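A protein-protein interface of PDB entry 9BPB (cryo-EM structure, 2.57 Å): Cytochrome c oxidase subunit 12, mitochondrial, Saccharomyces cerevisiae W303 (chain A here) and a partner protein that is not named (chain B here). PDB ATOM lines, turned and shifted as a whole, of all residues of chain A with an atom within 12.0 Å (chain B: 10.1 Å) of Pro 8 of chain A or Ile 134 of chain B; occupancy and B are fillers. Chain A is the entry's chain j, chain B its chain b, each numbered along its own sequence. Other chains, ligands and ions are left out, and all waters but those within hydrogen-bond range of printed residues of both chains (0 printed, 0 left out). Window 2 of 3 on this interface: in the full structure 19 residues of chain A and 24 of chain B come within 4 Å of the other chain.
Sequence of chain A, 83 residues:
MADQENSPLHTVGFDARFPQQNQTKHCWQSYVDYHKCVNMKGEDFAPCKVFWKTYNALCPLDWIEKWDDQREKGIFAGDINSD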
ATOM      1  N   PRO A   8      -9.324  21.004   7.720  1.00  0.00           N
ATOM      2  CA  PRO A   8      -9.902  20.002   6.820  1.00  0.00           C
ATOM      3  C   PRO A   8     -11.124  20.524   6.070  1.00  0.00           C
ATOM      4  O   PRO A   8     -11.863  19.740   5.473  1.00  0.00           O
ATOM      5  CB  PRO A   8     -10.288  18.867   7.770  1.00  0.00           C
ATOM      6  CG  PRO A   8     -10.582  19.551   9.057  1.00  0.00           C
ATOM      7  CD  PRO A   8      -9.676  20.755   9.128  1.00  0.00           C
ATOM      8  N   LEU A   9     -11.332  21.836   6.109  1.00  0.00           N
ATOM      9  CA  LEU A   9     -12.449  22.461   5.421  1.00  0.00           C
ATOM     10  C   LEU A   9     -12.014  22.994   4.062  1.00  0.00           C
ATOM     11  O   LEU A   9     -10.919  23.544   3.909  1.00  0.00           O
ATOM     12  CB  LEU A   9     -13.039  23.599   6.257  1.00  0.00           C
ATOM     13  CG  LEU A   9     -14.138  23.274   7.275  1.00  0.00           C
ATOM     14  CD1 LEU A   9     -13.696  22.213   8.270  1.00  0.00           C
ATOM     15  CD2 LEU A   9     -14.584  24.538   8.000  1.00  0.00           C
ATOM     16  N   HIS A  10     -12.885  22.823   3.072  1.00  0.00           N
ATOM     17  CA  HIS A  10     -12.664  23.366   1.739  1.00  0.00           C
ATOM     18  C   HIS A  10     -14.013  23.471   1.043  1.00  0.00           C
ATOM     19  O   HIS A  10     -15.003  22.876   1.474  1.00  0.00           O
ATOM     20  CB  HIS A  10     -11.691  22.502   0.929  1.00  0.00           C
ATOM     21  CG  HIS A  10     -12.219  21.141   0.605  1.00  0.00           C
ATOM     22  ND1 HIS A  10     -12.200  20.099   1.506  1.00  0.00           N
ATOM     23  CD2 HIS A  10     -12.778  20.649  -0.526  1.00  0.00           C
ATOM     24  CE1 HIS A  10     -12.727  19.025   0.947  1.00  0.00           C
ATOM     25  NE2 HIS A  10     -13.086  19.332  -0.287  1.00  0.00           N
ATOM     26  N   THR A  11     -14.043  24.243  -0.039  1.00  0.00           N
ATOM     27  CA  THR A  11     -15.267  24.443  -0.802  1.00  0.00           C
ATOM     28  C   THR A  11     -14.893  24.907  -2.204  1.00  0.00           C
ATOM     29  O   THR A  11     -13.714  25.022  -2.550  1.00  0.00           O
ATOM     30  CB  THR A  11     -16.197  25.443  -0.112  1.00  0.00           C
ATOM     31  OG1 THR A  11     -17.402  25.584  -0.873  1.00  0.00           O
ATOM     32  CG2 THR A  11     -15.527  26.792  -0.001  1.00  0.00           C
ATOM     33  N   VAL A  12     -15.920  25.170  -3.014  1.00  0.00           N
ATOM     34  CA  VAL A  12     -15.715  25.553  -4.404  1.00  0.00           C
ATOM     35  C   VAL A  12     -14.973  26.884  -4.477  1.00  0.00           C
ATOM     36  O   VAL A  12     -15.204  27.799  -3.677  1.00  0.00           O
ATOM     37  CB  VAL A  12     -17.071  25.626  -5.132  1.00  0.00           C
ATOM     38  CG1 VAL A  12     -16.884  25.992  -6.596  1.00  0.00           C
ATOM     39  CG2 VAL A  12     -17.816  24.308  -4.991  1.00  0.00           C
ATOM     40  N   TRP A  52     -20.062  17.218 -10.044  1.00  0.00           N
ATOM     41  CA  TRP A  52     -20.946  16.521  -9.112  1.00  0.00           C
ATOM     42  C   TRP A  52     -20.812  17.076  -7.701  1.00  0.00           C
ATOM     43  O   TRP A  52     -21.804  17.181  -6.971  1.00  0.00           O
ATOM     44  CB  TRP A  52     -20.655  15.024  -9.128  1.00  0.00           C
ATOM     45  CG  TRP A  52     -21.412  14.261  -8.091  1.00  0.00           C
ATOM     46  CD1 TRP A  52     -22.636  13.681  -8.238  1.00  0.00           C
ATOM     47  CD2 TRP A  52     -20.998  13.988  -6.747  1.00  0.00           C
ATOM     48  NE1 TRP A  52     -23.014  13.067  -7.073  1.00  0.00           N
ATOM     49  CE2 TRP A  52     -22.026  13.239  -6.140  1.00  0.00           C
ATOM     50  CE3 TRP A  52     -19.860  14.304  -5.997  1.00  0.00           C
ATOM     51  CZ2 TRP A  52     -21.950  12.802  -4.822  1.00  0.00           C
ATOM     52  CZ3 TRP A  52     -19.788  13.867  -4.686  1.00  0.00           C
ATOM     53  CH2 TRP A  52     -20.827  13.126  -4.112  1.00  0.00           C
ATOM     54  N   LYS A  53     -19.594  17.425  -7.293  1.00  0.00           N
ATOM     55  CA  LYS A  53     -19.411  18.100  -6.017  1.00  0.00           C
ATOM     56  C   LYS A  53     -19.718  19.590  -6.102  1.00  0.00           C
ATOM     57  O   LYS A  53     -19.693  20.277  -5.075  1.00  0.00           O
ATOM     58  CB  LYS A  53     -17.986  17.885  -5.501  1.00  0.00           C
ATOM     59  CG  LYS A  53     -16.903  18.528  -6.345  1.00  0.00           C
ATOM     60  CD  LYS A  53     -15.586  18.580  -5.592  1.00  0.00           C
ATOM     61  CE  LYS A  53     -14.452  19.061  -6.482  1.00  0.00           C
ATOM     62  NZ  LYS A  53     -13.194  19.284  -5.717  1.00  0.00           N
ATOM     63  N   THR A  54     -20.003  20.102  -7.301  1.00  0.00           N
ATOM     64  CA  THR A  54     -20.281  21.519  -7.480  1.00  0.00           C
ATOM     65  C   THR A  54     -21.772  21.831  -7.534  1.00  0.00           C
ATOM     66  O   THR A  54     -22.173  22.925  -7.118  1.00  0.00           O
ATOM     67  CB  THR A  54     -19.593  22.028  -8.753  1.00  0.00           C
ATOM     68  OG1 THR A  54     -18.205  21.671  -8.715  1.00  0.00           O
ATOM     69  CG2 THR A  54     -19.702  23.537  -8.868  1.00  0.00           C
ATOM     70  N   ASN A  56     -24.133  19.501  -6.195  1.00  0.00           N
ATOM     71  CA  ASN A  56     -24.555  19.043  -4.877  1.00  0.00           C
ATOM     72  C   ASN A  56     -24.295  20.123  -3.836  1.00  0.00           C
ATOM     73  O   ASN A  56     -24.986  20.198  -2.814  1.00  0.00           O
ATOM     74  CB  ASN A  56     -23.835  17.748  -4.511  1.00  0.00           C
ATOM     75  CG  ASN A  56     -24.452  16.537  -5.172  1.00  0.00           C
ATOM     76  OD1 ASN A  56     -25.585  16.163  -4.875  1.00  0.00           O
ATOM     77  ND2 ASN A  56     -23.712  15.922  -6.087  1.00  0.00           N
ATOM     78  N   ALA A  57     -23.291  20.958  -4.079  1.00  0.00           N
ATOM     79  CA  ALA A  57     -23.127  22.206  -3.360  1.00  0.00           C
ATOM     80  C   ALA A  57     -23.822  23.337  -4.114  1.00  0.00           C
ATOM     81  O   ALA A  57     -24.180  23.208  -5.289  1.00  0.00           O
ATOM     82  CB  ALA A  57     -21.646  22.522  -3.161  1.00  0.00           C
ATOM     83  N   LEU A  58     -24.058  24.442  -3.408  1.00  0.00           N
ATOM     84  CA  LEU A  58     -24.478  25.691  -4.034  1.00  0.00           C
ATOM     85  C   LEU A  58     -25.888  25.613  -4.622  1.00  0.00           C
ATOM     86  O   LEU A  58     -26.414  26.622  -5.102  1.00  0.00           O
ATOM     87  CB  LEU A  58     -23.459  26.089  -5.110  1.00  0.00           C
ATOM     88  CG  LEU A  58     -23.570  27.398  -5.897  1.00  0.00           C
ATOM     89  CD1 LEU A  58     -23.103  28.583  -5.071  1.00  0.00           C
ATOM     90  CD2 LEU A  58     -22.778  27.296  -7.187  1.00  0.00           C
ATOM     91  N   PRO B 113     -12.969  30.844  -0.017  1.00  0.00           N
ATOM     92  CA  PRO B 113     -13.745  30.458   1.163  1.00  0.00           C
ATOM     93  C   PRO B 113     -13.390  29.032   1.573  1.00  0.00           C
ATOM     94  O   PRO B 113     -12.551  28.375   0.963  1.00  0.00           O
ATOM     95  CB  PRO B 113     -15.190  30.575   0.677  1.00  0.00           C
ATOM     96  CG  PRO B 113     -15.105  30.255  -0.773  1.00  0.00           C
ATOM     97  CD  PRO B 113     -13.772  30.777  -1.251  1.00  0.00           C
ATOM     98  N   ALA B 114     -14.053  28.553   2.631  1.00  0.00           N
ATOM     99  CA  ALA B 114     -13.750  27.243   3.184  1.00  0.00           C
ATOM    100  C   ALA B 114     -14.956  26.333   3.355  1.00  0.00           C
ATOM    101  O   ALA B 114     -14.768  25.115   3.432  1.00  0.00           O
ATOM    102  CB  ALA B 114     -13.050  27.383   4.544  1.00  0.00           C
ATOM    103  N   MET B 115     -16.172  26.872   3.420  1.00  0.00           N
ATOM    104  CA  MET B 115     -17.368  26.055   3.576  1.00  0.00           C
ATOM    105  C   MET B 115     -18.604  26.920   3.364  1.00  0.00           C
ATOM    106  O   MET B 115     -18.650  28.065   3.817  1.00  0.00           O
ATOM    107  CB  MET B 115     -17.378  25.359   4.949  1.00  0.00           C
ATOM    108  CG  MET B 115     -17.204  26.268   6.157  1.00  0.00           C
ATOM    109  SD  MET B 115     -18.709  27.016   6.778  1.00  0.00           S
ATOM    110  CE  MET B 115     -19.490  25.577   7.498  1.00  0.00           C
ATOM    111  N   THR B 116     -19.594  26.363   2.666  1.00  0.00           N
ATOM    112  CA  THR B 116     -20.746  27.108   2.176  1.00  0.00           C
ATOM    113  C   THR B 116     -22.022  26.623   2.854  1.00  0.00           C
ATOM    114  O   THR B 116     -22.218  25.418   3.041  1.00  0.00           O
ATOM    115  CB  THR B 116     -20.883  26.962   0.651  1.00  0.00           C
ATOM    116  OG1 THR B 116     -19.684  27.423   0.016  1.00  0.00           O
ATOM    117  CG2 THR B 116     -22.059  27.775   0.131  1.00  0.00           C
ATOM    118  N   TYR B 130     -26.490  22.228   4.800  1.00  0.00           N
ATOM    119  CA  TYR B 130     -25.054  22.362   4.570  1.00  0.00           C
ATOM    120  C   TYR B 130     -24.680  21.453   3.409  1.00  0.00           C
ATOM    121  O   TYR B 130     -24.585  20.233   3.547  1.00  0.00           O
ATOM    122  CB  TYR B 130     -24.263  22.023   5.828  1.00  0.00           C
ATOM    123  CG  TYR B 130     -24.493  22.950   7.004  1.00  0.00           C
ATOM    124  CD1 TYR B 130     -25.360  24.032   6.917  1.00  0.00           C
ATOM    125  CD2 TYR B 130     -23.823  22.748   8.201  1.00  0.00           C
ATOM    126  CE1 TYR B 130     -25.563  24.872   7.990  1.00  0.00           C
ATOM    127  CE2 TYR B 130     -24.018  23.584   9.278  1.00  0.00           C
ATOM    128  CZ  TYR B 130     -24.888  24.644   9.168  1.00  0.00           C
ATOM    129  OH  TYR B 130     -25.082  25.479  10.242  1.00  0.00           O
ATOM    130  N   SER B 131     -24.450  22.065   2.249  1.00  0.00           N
ATOM    131  CA  SER B 131     -24.185  21.306   1.036  1.00  0.00           C
ATOM    132  C   SER B 131     -22.794  20.685   1.022  1.00  0.00           C
ATOM    133  O   SER B 131     -22.545  19.774   0.225  1.00  0.00           O
ATOM    134  CB  SER B 131     -24.374  22.216  -0.173  1.00  0.00           C
ATOM    135  OG  SER B 131     -23.349  23.191  -0.244  1.00  0.00           O
ATOM    136  N   ASP B 132     -21.884  21.153   1.872  1.00  0.00           N
ATOM    137  CA  ASP B 132     -20.550  20.572   1.945  1.00  0.00           C
ATOM    138  C   ASP B 132     -20.622  19.145   2.475  1.00  0.00           C
ATOM    139  O   ASP B 132     -21.502  18.806   3.270  1.00  0.00           O
ATOM    140  CB  ASP B 132     -19.647  21.418   2.839  1.00  0.00           C
ATOM    141  CG  ASP B 132     -20.324  21.822   4.136  1.00  0.00           C
ATOM    142  OD1 ASP B 132     -21.530  21.539   4.291  1.00  0.00           O
ATOM    143  OD2 ASP B 132     -19.651  22.418   5.003  1.00  0.00           O
ATOM    144  N   PHE B 133     -19.685  18.310   2.035  1.00  0.00           N
ATOM    145  CA  PHE B 133     -19.640  16.901   2.424  1.00  0.00           C
ATOM    146  C   PHE B 133     -18.417  16.580   3.271  1.00  0.00           C
ATOM    147  O   PHE B 133     -17.785  15.533   3.096  1.00  0.00           O
ATOM    148  CB  PHE B 133     -19.688  16.009   1.190  1.00  0.00           C
ATOM    149  CG  PHE B 133     -20.911  16.212   0.348  1.00  0.00           C
ATOM    150  CD1 PHE B 133     -22.169  16.222   0.926  1.00  0.00           C
ATOM    151  CD2 PHE B 133     -20.808  16.392  -1.020  1.00  0.00           C
ATOM    152  CE1 PHE B 133     -23.298  16.414   0.156  1.00  0.00           C
ATOM    153  CE2 PHE B 133     -21.934  16.581  -1.793  1.00  0.00           C
ATOM    154  CZ  PHE B 133     -23.180  16.592  -1.205  1.00  0.00           C
ATOM    155  N   ILE B 134     -18.058  17.473   4.195  1.00  0.00           N
ATOM    156  CA  ILE B 134     -16.951  17.200   5.103  1.00  0.00           C
ATOM    157  C   ILE B 134     -17.329  16.101   6.090  1.00  0.00           C
ATOM    158  O   ILE B 134     -16.477  15.316   6.528  1.00  0.00           O
ATOM    159  CB  ILE B 134     -16.531  18.494   5.826  1.00  0.00           C
ATOM    160  CG1 ILE B 134     -16.172  19.577   4.807  1.00  0.00           C
ATOM    161  CG2 ILE B 134     -15.358  18.236   6.757  1.00  0.00           C
ATOM    162  CD1 ILE B 134     -15.045  19.188   3.875  1.00  0.00           C
ATOM    163  N   ASN B 135     -18.608  16.020   6.446  1.00  0.00           N
ATOM    164  CA  ASN B 135     -19.065  15.040   7.422  1.00  0.00           C
ATOM    165  C   ASN B 135     -18.887  13.620   6.894  1.00  0.00           C
ATOM    166  O   ASN B 135     -18.966  13.365   5.690  1.00  0.00           O
ATOM    167  CB  ASN B 135     -20.532  15.295   7.774  1.00  0.00           C
ATOM    168  CG  ASN B 135     -21.050  14.345   8.832  1.00  0.00           C
ATOM    169  OD1 ASN B 135     -20.302  13.902   9.703  1.00  0.00           O
ATOM    170  ND2 ASN B 135     -22.338  14.032   8.768  1.00  0.00           N
ATOM    171  N   ASP B 136     -18.641  12.689   7.818  1.00  0.00           N
ATOM    172  CA  ASP B 136     -18.429  11.291   7.462  1.00  0.00           C
ATOM    173  C   ASP B 136     -19.673  10.626   6.893  1.00  0.00           C
ATOM    174  O   ASP B 136     -19.560   9.550   6.297  1.00  0.00           O
ATOM    175  CB  ASP B 136     -17.939  10.508   8.679  1.00  0.00           C
ATOM    176  CG  ASP B 136     -16.463  10.716   8.952  1.00  0.00           C
ATOM    177  OD1 ASP B 136     -15.699  10.905   7.981  1.00  0.00           O
ATOM    178  OD2 ASP B 136     -16.065  10.693  10.135  1.00  0.00           O
ATOM    179  N   SER B 137     -20.850  11.230   7.063  1.00  0.00           N
ATOM    180  CA  SER B 137     -22.061  10.683   6.463  1.00  0.00           C
ATOM    181  C   SER B 137     -22.079  10.849   4.950  1.00  0.00           C
ATOM    182  O   SER B 137     -22.637   9.995   4.253  1.00  0.00           O
ATOM    183  CB  SER B 137     -23.297  11.346   7.071  1.00  0.00           C
ATOM    184  OG  SER B 137     -24.482  10.885   6.446  1.00  0.00           O
ATOM    185  N   GLY B 138     -21.486  11.921   4.429  1.00  0.00           N
ATOM    186  CA  GLY B 138     -21.542  12.180   3.005  1.00  0.00           C
ATOM    187  C   GLY B 138     -22.868  12.718   2.527  1.00  0.00           C
ATOM    188  O   GLY B 138     -23.086  12.826   1.319  1.00  0.00           O
ATOM    189  N   GLU B 139     -23.761  13.068   3.450  1.00  0.00           N
ATOM    190  CA  GLU B 139     -25.091  13.553   3.122  1.00  0.00           C
ATOM    191  C   GLU B 139     -25.258  14.967   3.654  1.00  0.00           C
ATOM    192  O   GLU B 139     -24.636  15.350   4.648  1.00  0.00           O
ATOM    193  CB  GLU B 139     -26.179  12.650   3.719  1.00  0.00           C
ATOM    194  CG  GLU B 139     -26.137  11.214   3.233  1.00  0.00           C
ATOM    195  CD  GLU B 139     -26.909  10.277   4.138  1.00  0.00           C
ATOM    196  OE1 GLU B 139     -28.000  10.662   4.606  1.00  0.00           O
ATOM    197  OE2 GLU B 139     -26.422   9.155   4.389  1.00  0.00           O
ATOM    198  N   THR B 140     -26.099  15.742   2.978  1.00  0.00           N
ATOM    199  CA  THR B 140     -26.398  17.087   3.443  1.00  0.00           C
ATOM    200  C   THR B 140     -27.189  17.028   4.743  1.00  0.00           C
ATOM    201  O   THR B 140     -28.015  16.134   4.945  1.00  0.00           O
ATOM    202  CB  THR B 140     -27.187  17.856   2.388  1.00  0.00           C
ATOM    203  OG1 THR B 140     -28.431  17.192   2.141  1.00  0.00           O
ATOM    204  CG2 THR B 140     -26.400  17.936   1.091  1.00  0.00           C
ATOM    205  N   VAL B 141     -26.929  17.983   5.628  1.00  0.00           N
ATOM    206  CA  VAL B 141     -27.631  18.093   6.899  1.00  0.00           C
ATOM    207  C   VAL B 141     -28.603  19.257   6.784  1.00  0.00           C
ATOM    208  O   VAL B 141     -28.193  20.412   6.622  1.00  0.00           O
ATOM    209  CB  VAL B 141     -26.665  18.268   8.079  1.00  0.00           C
ATOM    210  CG1 VAL B 141     -25.992  16.947   8.400  1.00  0.00           C
ATOM    211  CG2 VAL B 141     -25.609  19.311   7.764  1.00  0.00           C
ATOM    212  N   PRO B 170     -18.177  27.884  12.352  1.00  0.00           N
ATOM    213  CA  PRO B 170     -16.889  27.938  13.058  1.00  0.00           C
ATOM    214  C   PRO B 170     -16.321  29.345  13.102  1.00  0.00           C
ATOM    215  O   PRO B 170     -16.773  30.220  12.358  1.00  0.00           O
ATOM    216  CB  PRO B 170     -15.988  27.004  12.236  1.00  0.00           C
ATOM    217  CG  PRO B 170     -16.888  26.314  11.259  1.00  0.00           C
ATOM    218  CD  PRO B 170     -18.058  27.209  11.052  1.00  0.00           C
ATOM    219  N   THR B 173     -13.081  31.458  10.116  1.00  0.00           N
ATOM    220  CA  THR B 173     -13.351  30.736   8.883  1.00  0.00           C
ATOM    221  C   THR B 173     -14.064  31.646   7.892  1.00  0.00           C
ATOM    222  O   THR B 173     -14.947  32.422   8.272  1.00  0.00           O
ATOM    223  CB  THR B 173     -14.202  29.488   9.154  1.00  0.00           C
ATOM    224  OG1 THR B 173     -13.603  28.721  10.206  1.00  0.00           O
ATOM    225  CG2 THR B 173     -14.306  28.625   7.908  1.00  0.00           C
ATOM    226  N   LEU B 241     -13.304  25.851  16.096  1.00  0.00           N
ATOM    227  CA  LEU B 241     -13.185  24.889  15.001  1.00  0.00           C
ATOM    228  C   LEU B 241     -13.387  23.446  15.448  1.00  0.00           C
ATOM    229  O   LEU B 241     -14.101  22.707  14.749  1.00  0.00           O
ATOM    230  CB  LEU B 241     -11.840  25.073  14.291  1.00  0.00           C
ATOM    231  CG  LEU B 241     -11.647  24.278  12.996  1.00  0.00           C
ATOM    232  CD1 LEU B 241     -12.886  24.357  12.115  1.00  0.00           C
ATOM    233  CD2 LEU B 241     -10.421  24.768  12.244  1.00  0.00           C
ATOM    234  N   PRO B 242     -12.798  22.970  16.554  1.00  0.00           N
ATOM    235  CA  PRO B 242     -13.131  21.607  17.003  1.00  0.00           C
ATOM    236  C   PRO B 242     -14.615  21.403  17.258  1.00  0.00           C
ATOM    237  O   PRO B 242     -15.238  20.568  16.596  1.00  0.00           O
ATOM    238  CB  PRO B 242     -12.294  21.449  18.280  1.00  0.00           C
ATOM    239  CG  PRO B 242     -11.156  22.370  18.096  1.00  0.00           C
ATOM    240  CD  PRO B 242     -11.715  23.554  17.367  1.00  0.00           C
ATOM    241  N   PHE B 244     -17.256  22.682  16.333  1.00  0.00           N
ATOM    242  CA  PHE B 244     -18.084  22.603  15.135  1.00  0.00           C
ATOM    243  C   PHE B 244     -18.053  21.199  14.542  1.00  0.00           C
ATOM    244  O   PHE B 244     -19.047  20.738  13.971  1.00  0.00           O
ATOM    245  CB  PHE B 244     -17.614  23.643  14.116  1.00  0.00           C
ATOM    246  CG  PHE B 244     -18.222  23.490  12.753  1.00  0.00           C
ATOM    247  CD1 PHE B 244     -19.503  23.940  12.499  1.00  0.00           C
ATOM    248  CD2 PHE B 244     -17.504  22.912  11.721  1.00  0.00           C
ATOM    249  CE1 PHE B 244     -20.063  23.811  11.244  1.00  0.00           C
ATOM    250  CE2 PHE B 244     -18.058  22.777  10.465  1.00  0.00           C
ATOM    251  CZ  PHE B 244     -19.340  23.229  10.227  1.00  0.00           C
ATOM    252  N   LEU B 245     -16.918  20.506  14.669  1.00  0.00           N
ATOM    253  CA  LEU B 245     -16.781  19.177  14.078  1.00  0.00           C
ATOM    254  C   LEU B 245     -17.530  18.120  14.883  1.00  0.00           C
ATOM    255  O   LEU B 245     -18.115  17.197  14.305  1.00  0.00           O
ATOM    256  CB  LEU B 245     -15.303  18.813  13.948  1.00  0.00           C
ATOM    257  CG  LEU B 245     -14.548  19.551  12.840  1.00  0.00           C
ATOM    258  CD1 LEU B 245     -13.050  19.345  12.970  1.00  0.00           C
ATOM    259  CD2 LEU B 245     -15.036  19.094  11.475  1.00  0.00           C
ATOM    260  N   GLU B 246     -17.520  18.223  16.216  1.00  0.00           N
ATOM    261  CA  GLU B 246     -18.335  17.314  17.016  1.00  0.00           C
ATOM    262  C   GLU B 246     -19.797  17.728  17.067  1.00  0.00           C
ATOM    263  O   GLU B 246     -20.564  17.131  17.828  1.00  0.00           O
ATOM    264  CB  GLU B 246     -17.797  17.181  18.444  1.00  0.00           C
ATOM    265  CG  GLU B 246     -16.464  16.446  18.569  1.00  0.00           C
ATOM    266  CD  GLU B 246     -15.268  17.337  18.337  1.00  0.00           C
ATOM    267  OE1 GLU B 246     -15.469  18.549  18.158  1.00  0.00           O
ATOM    268  OE2 GLU B 246     -14.130  16.826  18.337  1.00  0.00           O
ATOM    269  N   LEU B 248     -21.367  18.772  13.739  1.00  0.00           N
ATOM    270  CA  LEU B 248     -21.835  18.410  12.406  1.00  0.00           C
ATOM    271  C   LEU B 248     -21.937  16.900  12.243  1.00  0.00           C
ATOM    272  O   LEU B 248     -22.844  16.404  11.567  1.00  0.00           O
ATOM    273  CB  LEU B 248     -20.903  19.004  11.352  1.00  0.00           C
ATOM    274  CG  LEU B 248     -21.399  18.941   9.909  1.00  0.00           C
ATOM    275  CD1 LEU B 248     -22.499  19.956   9.701  1.00  0.00           C
ATOM    276  CD2 LEU B 248     -20.256  19.185   8.943  1.00  0.00           C
ATOM    277  N   ASN B 249     -21.010  16.155  12.847  1.00  0.00           N
ATOM    278  CA  ASN B 249     -21.052  14.700  12.752  1.00  0.00           C
ATOM    279  C   ASN B 249     -22.289  14.133  13.438  1.00  0.00           C
ATOM    280  O   ASN B 249     -22.919  13.200  12.927  1.00  0.00           O
ATOM    281  CB  ASN B 249     -19.781  14.102  13.353  1.00  0.00           C
ATOM    282  CG  ASN B 249     -19.442  12.744  12.772  1.00  0.00           C
ATOM    283  OD1 ASN B 249     -20.229  12.157  12.030  1.00  0.00           O
ATOM    284  ND2 ASN B 249     -18.262  12.237  13.108  1.00  0.00           N
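OG1 of Thr 116 of chain B lies within hydrogen-bond range of OG1 of Thr 11 of chain A (3.1 Å). O of Ala 114 of chain B sits at hydrogen-bond distance from N of His 10 of chain A, at 3.0 Å. The side-chain hydroxyl (OG) of Ser 131 of chain B lies within hydrogen-bond range of the backbone NH (N) of Leu 58 of chain A (3.5 Å).
ND2 of Asn 56 of chain A sits at hydrogen-bond distance from O of Trp 52 of chain A.
Among the printed residues, merely in contact across the chains: Ala 57 of chain A with Ser 131 of chain B (3.3 Å), Asn 56 of chain A with Ser 131 of chain B (3.4 Å), Thr 11 of chain A with Ala 114 of chain B (3.4 Å), Thr 11 of chain A with Pro 113 of chain B (3.5 Å), Thr 11 of chain A with Met 115 of chain B (3.5 Å), Asn 56 of chain A with Phe 133 of chain B (3.5 Å), Leu 9 of chain A with Ala 114 of chain B (3.5 Å), Pro 8 of chain A with Ile 134 of chain B (3.6 Å), Leu 9 of chain A with Met 115 of chain B (3.6 Å), His 10 of chain A with Ile 134 of chain B (3.7 Å) and Val 12 of chain A with Pro 113 of chain B (3.8 Å).
Of chain B, only Ile 134 (3.6 Å) comes within 4 Å of Pro 8 of chain A. Printed residues of chain B within 4 Å of Leu 9 of chain A: Ala 114 and Met 115. His 10 of chain A touches just these residues of chain B: Ala 114 and Ile 134. Of the printed residues of chain B, Thr 11 of chain A touches Pro 113 (3.5 Å), Ala 114 (3.4 Å), Met 115 (3.5 Å) and Thr 116 (3.1 Å). Printed residues of chain B within 4 Å of Ala 57 of chain A: Ser 131 (3.3 Å). Of the printed residues of chain B, Leu 58 of chain A touches Ser 131. Of the printed residues of chain A, Pro 113 of chain B touches Thr 11 and Val 12. Of the printed residues of chain A, Met 115 of chain B touches Leu 9 and Thr 11. No residue of chain A comes within 4 Å of Asp 132 of chain B. Printed residues of chain A within 4 Å of Ile 134 of chain B: Pro 8 and His 10. No residue of chain A comes within 4 Å of Asp 136 of chain B. Gly 138 of chain B touches none of the printed residues of chain A. Val 141 of chain B touches none of the printed residues of chain A. Phe 244 of chain B touches none of the printed residues of chain A.
Of the 25 printed residues of chain B, 7 touch a printed residue of chain A. Hydrophobic or aromatic side chains of chain B within 4 Å of the printed part of chain A: Pro 113, Met 115, Phe 133 and Ile 134. Hydrophobic or aromatic side chains of chain A that line the printed part of chain B: Leu 9, His 10 and Ala 57. Among the printed residues, no Asp or Glu carboxylate lies within 4 Å of a Lys or Arg side-chain nitrogen of the other chain.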
